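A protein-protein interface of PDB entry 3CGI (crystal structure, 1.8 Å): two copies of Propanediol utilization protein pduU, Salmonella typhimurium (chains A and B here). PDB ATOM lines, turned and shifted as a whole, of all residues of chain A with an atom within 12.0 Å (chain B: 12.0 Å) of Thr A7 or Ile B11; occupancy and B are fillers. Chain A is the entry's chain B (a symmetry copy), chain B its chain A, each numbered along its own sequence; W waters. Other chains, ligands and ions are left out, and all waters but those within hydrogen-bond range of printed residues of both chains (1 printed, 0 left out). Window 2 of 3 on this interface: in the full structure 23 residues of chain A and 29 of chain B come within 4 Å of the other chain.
N of Ile B11 is in hydrogen-bond range of O of Asp A8, 2.8 Å away. The backbone carbonyl oxygen (O) of Ile B11 is in hydrogen-bond range of the backbone NH (N) of Met A10. The side-chain carboxylate (OE2) of Glu B13 lies within salt-bridge range of the guanidinium group (NE) of Arg A9 (2.9 Å). O of Met A10 sits at hydrogen-bond distance from N of Glu B13 (2.8 Å). N of Gln A12 lies within hydrogen-bond range of O of Glu B13 (2.8 Å). N of Val B15 lies within hydrogen-bond range of O of Gln A12.
Among the printed residues, pairs that only touch across the chains: Glu A13 with Val B15 (3.0 Å), Gln A12 with Gln B12 (3.1 Å), Asp A8 with Met B10 (3.2 Å), Met A10 with Gln B12 (3.3 Å), Met A10 with Met B10 (3.4 Å), Ile A11 with Glu B13 (3.4 Å), Arg A9 with Ile B11 (3.5 Å), Gln A12 with Tyr B14 (3.5 Å), Thr A7 with Ile B11 (3.7 Å), Ile A11 with Val B15 (3.9 Å) and Gln A12 with Met B10 (3.9 Å).
Of chain B, only Ile B11 (3.7 Å) comes within 4 Å of Thr A7. No residue of chain A comes within 4 Å of Arg B9. Printed residues of chain A within 4 Å of Met B10: Asp A8, Met A10 and Gln A12. Ile B11 touches just these residues of chain A: Thr A7, Asp A8, Arg A9 and Met A10. Of the printed residues of chain A, Val B15 touches Ile A11 (3.9 Å), Gln A12 (3.2 Å) and Glu A13 (3.0 Å). The nearest residue of chain B that does not touch Thr A7 is Met B10 (4.1 Å).
Of the 7 printed residues of chain A, 7 touch a printed residue of chain B. Printed residues of chain A that touch a printed residue of chain B: Thr A7, Asp A8, Arg A9, Met A10, Ile A11, Gln A12 and Glu A13. Hydrophobic or aromatic side chains of chain A within 4 Å of the printed part of chain B: Met A10 and Ile A11. Among the printed residues, 17 pairs touch across the chains. Among the printed residues, Asp or Glu carboxylates within 4 Å of a Lys or Arg side-chain nitrogen of the other chain: Arg A9 with Glu B13.
Arg A9 touches Ile B11, but with the chains exchanged Ile A11 does not touch Arg B9 (11.8 Å). Met A10 touches Glu B13, but with the chains exchanged Glu A13 does not touch Met B10 (10.3 Å). Ile A11 touches Glu B13, but with the chains exchanged Glu A13 does not touch Ile B11 (10.1 Å). Gln B12 touches its own counterpart, Gln A12.
Water W1 bridges OE1 of Glu B13 (3.0 Å) and NH1 of Arg A9 (3.2 Å).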
ATOM      1  N   THR A   7      29.847 -22.313  10.557  1.00  0.00           N
ATOM      2  CA  THR A   7      29.259 -20.949  10.478  1.00  0.00           C
ATOM      3  C   THR A   7      30.368 -19.892  10.562  1.00  0.00           C
ATOM      4  O   THR A   7      31.124 -19.855  11.539  1.00  0.00           O
ATOM      5  CB  THR A   7      28.231 -20.702  11.616  1.00  0.00           C
ATOM      6  OG1 THR A   7      27.306 -21.794  11.685  1.00  0.00           O
ATOM      7  CG2 THR A   7      27.459 -19.414  11.373  1.00  0.00           C
ATOM      8  N   ASP A   8      30.460 -19.045   9.531  1.00  0.00           N
ATOM      9  CA  ASP A   8      31.449 -17.957   9.494  1.00  0.00           C
ATOM     10  C   ASP A   8      31.219 -16.938  10.614  1.00  0.00           C
ATOM     11  O   ASP A   8      30.088 -16.736  11.073  1.00  0.00           O
ATOM     12  CB  ASP A   8      31.473 -17.261   8.125  1.00  0.00           C
ATOM     13  CG  ASP A   8      32.383 -17.972   7.114  1.00  0.00           C
ATOM     14  OD1 ASP A   8      32.741 -19.154   7.327  1.00  0.00           O
ATOM     15  OD2 ASP A   8      32.748 -17.334   6.103  1.00  0.00           O
ATOM     16  N   ARG A   9      32.309 -16.293  11.027  1.00  0.00           N
ATOM     17  CA  ARG A   9      32.302 -15.427  12.197  1.00  0.00           C
ATOM     18  C   ARG A   9      33.033 -14.105  11.920  1.00  0.00           C
ATOM     19  O   ARG A   9      34.078 -14.082  11.264  1.00  0.00           O
ATOM     20  CB  ARG A   9      32.977 -16.192  13.330  1.00  0.00           C
ATOM     21  CG  ARG A   9      32.594 -15.776  14.717  1.00  0.00           C
ATOM     22  CD  ARG A   9      33.254 -16.688  15.758  1.00  0.00           C
ATOM     23  NE  ARG A   9      32.996 -16.143  17.084  1.00  0.00           N
ATOM     24  CZ  ARG A   9      32.045 -16.549  17.923  1.00  0.00           C
ATOM     25  NH1 ARG A   9      31.925 -15.926  19.082  1.00  0.00           N
ATOM     26  NH2 ARG A   9      31.251 -17.576  17.649  1.00  0.00           N
ATOM     27  N   MET A  10      32.483 -12.999  12.419  1.00  0.00           N
ATOM     28  CA  MET A  10      33.087 -11.696  12.189  1.00  0.00           C
ATOM     29  C   MET A  10      32.801 -10.774  13.354  1.00  0.00           C
ATOM     30  O   MET A  10      31.767 -10.885  14.018  1.00  0.00           O
ATOM     31  CB  MET A  10      32.533 -11.097  10.901  1.00  0.00           C
ATOM     32  CG  MET A  10      33.312  -9.909  10.371  1.00  0.00           C
ATOM     33  SD  MET A  10      32.815  -9.487   8.677  1.00  0.00           S
ATOM     34  CE  MET A  10      31.067  -9.199   8.961  1.00  0.00           C
ATOM     35  N   ILE A  11      33.746  -9.892  13.636  1.00  0.00           N
ATOM     36  CA  ILE A  11      33.506  -8.863  14.638  1.00  0.00           C
ATOM     37  C   ILE A  11      32.879  -7.681  13.909  1.00  0.00           C
ATOM     38  O   ILE A  11      33.347  -7.271  12.854  1.00  0.00           O
ATOM     39  CB  ILE A  11      34.787  -8.429  15.350  1.00  0.00           C
ATOM     40  CG1 ILE A  11      35.438  -9.627  16.047  1.00  0.00           C
ATOM     41  CG2 ILE A  11      34.473  -7.342  16.396  1.00  0.00           C
ATOM     42  CD1 ILE A  11      36.821  -9.330  16.575  1.00  0.00           C
ATOM     43  N   GLN A  12      31.802  -7.138  14.460  1.00  0.00           N
ATOM     44  CA  GLN A  12      31.172  -5.986  13.847  1.00  0.00           C
ATOM     45  C   GLN A  12      31.136  -4.857  14.851  1.00  0.00           C
ATOM     46  O   GLN A  12      30.537  -4.992  15.905  1.00  0.00           O
ATOM     47  CB  GLN A  12      29.769  -6.326  13.343  1.00  0.00           C
ATOM     48  CG  GLN A  12      29.779  -7.335  12.195  1.00  0.00           C
ATOM     49  CD  GLN A  12      28.409  -7.558  11.590  1.00  0.00           C
ATOM     50  OE1 GLN A  12      28.070  -8.673  11.186  1.00  0.00           O
ATOM     51  NE2 GLN A  12      27.605  -6.505  11.540  1.00  0.00           N
ATOM     52  N   GLU A  13      31.833  -3.760  14.529  1.00  0.00           N
ATOM     53  CA  GLU A  13      31.834  -2.585  15.396  1.00  0.00           C
ATOM     54  C   GLU A  13      30.640  -1.791  14.968  1.00  0.00           C
ATOM     55  O   GLU A  13      30.554  -1.396  13.808  1.00  0.00           O
ATOM     56  CB  GLU A  13      33.059  -1.678  15.189  1.00  0.00           C
ATOM     57  CG  GLU A  13      34.371  -2.287  15.507  1.00  0.00           C
ATOM     58  CD  GLU A  13      35.530  -1.328  15.229  1.00  0.00           C
ATOM     59  OE1 GLU A  13      35.345  -0.082  15.258  1.00  0.00           O
ATOM     60  OE2 GLU A  13      36.624  -1.840  14.976  1.00  0.00           O
ATOM     61  N   THR B   7      19.010 -16.395   3.546  1.00  0.00           N
ATOM     62  CA  THR B   7      19.653 -17.735   3.337  1.00  0.00           C
ATOM     63  C   THR B   7      21.049 -17.843   3.978  1.00  0.00           C
ATOM     64  O   THR B   7      21.225 -18.617   4.925  1.00  0.00           O
ATOM     65  CB  THR B   7      19.722 -18.125   1.824  1.00  0.00           C
ATOM     66  OG1 THR B   7      20.525 -19.307   1.659  1.00  0.00           O
ATOM     67  CG2 THR B   7      20.303 -16.983   0.971  1.00  0.00           C
ATOM     68  N   ASP B   8      22.028 -17.086   3.464  1.00  0.00           N
ATOM     69  CA  ASP B   8      23.398 -17.104   3.997  1.00  0.00           C
ATOM     70  C   ASP B   8      23.421 -16.625   5.444  1.00  0.00           C
ATOM     71  O   ASP B   8      22.676 -15.728   5.835  1.00  0.00           O
ATOM     72  CB  ASP B   8      24.371 -16.296   3.132  1.00  0.00           C
ATOM     73  CG  ASP B   8      24.796 -17.046   1.866  1.00  0.00           C
ATOM     74  OD1 ASP B   8      24.100 -18.011   1.467  1.00  0.00           O
ATOM     75  OD2 ASP B   8      25.829 -16.670   1.266  1.00  0.00           O
ATOM     76  N   ARG B   9      24.309 -17.233   6.218  1.00  0.00           N
ATOM     77  CA  ARG B   9      24.288 -17.105   7.653  1.00  0.00           C
ATOM     78  C   ARG B   9      25.673 -16.804   8.234  1.00  0.00           C
ATOM     79  O   ARG B   9      26.677 -17.343   7.768  1.00  0.00           O
ATOM     80  CB  ARG B   9      23.768 -18.426   8.177  1.00  0.00           C
ATOM     81  CG  ARG B   9      23.247 -18.385   9.548  1.00  0.00           C
ATOM     82  CD  ARG B   9      22.570 -19.684   9.902  1.00  0.00           C
ATOM     83  NE  ARG B   9      22.029 -19.506  11.233  1.00  0.00           N
ATOM     84  CZ  ARG B   9      20.752 -19.305  11.532  1.00  0.00           C
ATOM     85  NH1 ARG B   9      20.440 -19.115  12.792  1.00  0.00           N
ATOM     86  NH2 ARG B   9      19.795 -19.332  10.609  1.00  0.00           N
ATOM     87  N   MET B  10      25.724 -15.950   9.255  1.00  0.00           N
ATOM     88  CA  MET B  10      26.997 -15.585   9.870  1.00  0.00           C
ATOM     89  C   MET B  10      26.810 -15.207  11.333  1.00  0.00           C
ATOM     90  O   MET B  10      25.736 -14.775  11.737  1.00  0.00           O
ATOM     91  CB  MET B  10      27.631 -14.428   9.086  1.00  0.00           C
ATOM     92  CG  MET B  10      29.078 -14.143   9.431  1.00  0.00           C
ATOM     93  SD  MET B  10      29.809 -12.891   8.359  1.00  0.00           S
ATOM     94  CE  MET B  10      28.662 -11.530   8.548  1.00  0.00           C
ATOM     95  N   ILE B  11      27.851 -15.423  12.126  1.00  0.00           N
ATOM     96  CA  ILE B  11      27.856 -14.999  13.517  1.00  0.00           C
ATOM     97  C   ILE B  11      28.527 -13.631  13.531  1.00  0.00           C
ATOM     98  O   ILE B  11      29.543 -13.420  12.866  1.00  0.00           O
ATOM     99  CB  ILE B  11      28.648 -15.961  14.420  1.00  0.00           C
ATOM    100  CG1 ILE B  11      28.034 -17.365  14.370  1.00  0.00           C
ATOM    101  CG2 ILE B  11      28.672 -15.437  15.872  1.00  0.00           C
ATOM    102  CD1 ILE B  11      28.887 -18.426  15.026  1.00  0.00           C
ATOM    103  N   GLN B  12      27.923 -12.686  14.247  1.00  0.00           N
ATOM    104  CA  GLN B  12      28.499 -11.355  14.404  1.00  0.00           C
ATOM    105  C   GLN B  12      28.768 -11.116  15.874  1.00  0.00           C
ATOM    106  O   GLN B  12      27.842 -11.162  16.685  1.00  0.00           O
ATOM    107  CB  GLN B  12      27.584 -10.232  13.870  1.00  0.00           C
ATOM    108  CG  GLN B  12      26.124 -10.278  14.328  1.00  0.00           C
ATOM    109  CD  GLN B  12      25.644  -8.971  14.935  1.00  0.00           C
ATOM    110  OE1 GLN B  12      24.649  -8.383  14.498  1.00  0.00           O
ATOM    111  NE2 GLN B  12      26.338  -8.524  15.964  1.00  0.00           N
ATOM    112  N   GLU B  13      30.037 -10.892  16.216  1.00  0.00           N
ATOM    113  CA  GLU B  13      30.409 -10.546  17.582  1.00  0.00           C
ATOM    114  C   GLU B  13      30.301  -9.059  17.614  1.00  0.00           C
ATOM    115  O   GLU B  13      31.040  -8.378  16.908  1.00  0.00           O
ATOM    116  CB  GLU B  13      31.847 -10.949  17.933  1.00  0.00           C
ATOM    117  CG  GLU B  13      32.133 -12.427  17.874  1.00  0.00           C
ATOM    118  CD  GLU B  13      33.600 -12.732  18.129  1.00  0.00           C
ATOM    119  OE1 GLU B  13      34.166 -12.193  19.097  1.00  0.00           O
ATOM    120  OE2 GLU B  13      34.197 -13.472  17.324  1.00  0.00           O
ATOM    121  N   TYR B  14      29.407  -8.526  18.429  1.00  0.00           N
ATOM    122  CA  TYR B  14      29.265  -7.101  18.448  1.00  0.00           C
ATOM    123  C   TYR B  14      30.164  -6.430  19.490  1.00  0.00           C
ATOM    124  O   TYR B  14      30.366  -6.949  20.595  1.00  0.00           O
ATOM    125  CB  TYR B  14      27.818  -6.699  18.645  1.00  0.00           C
ATOM    126  CG  TYR B  14      27.136  -7.231  19.880  1.00  0.00           C
ATOM    127  CD1 TYR B  14      26.351  -8.390  19.823  1.00  0.00           C
ATOM    128  CD2 TYR B  14      27.202  -6.540  21.076  1.00  0.00           C
ATOM    129  CE1 TYR B  14      25.675  -8.850  20.951  1.00  0.00           C
ATOM    130  CE2 TYR B  14      26.540  -6.993  22.195  1.00  0.00           C
ATOM    131  CZ  TYR B  14      25.792  -8.152  22.129  1.00  0.00           C
ATOM    132  OH  TYR B  14      25.133  -8.605  23.246  1.00  0.00           O
ATOM    133  N   VAL B  15      30.735  -5.301  19.077  1.00  0.00           N
ATOM    134  CA  VAL B  15      31.452  -4.388  19.968  1.00  0.00           C
ATOM    135  C   VAL B  15      31.098  -2.987  19.450  1.00  0.00           C
ATOM    136  O   VAL B  15      30.814  -2.827  18.243  1.00  0.00           O
ATOM    137  CB  VAL B  15      32.989  -4.627  19.973  1.00  0.00           C
ATOM    138  CG1 VAL B  15      33.346  -6.094  20.325  1.00  0.00           C
ATOM    139  CG2 VAL B  15      33.595  -4.256  18.665  1.00  0.00           C
HETATM  140  O   HOH W   1      32.314 -13.466  21.127  1.00  0.00           O
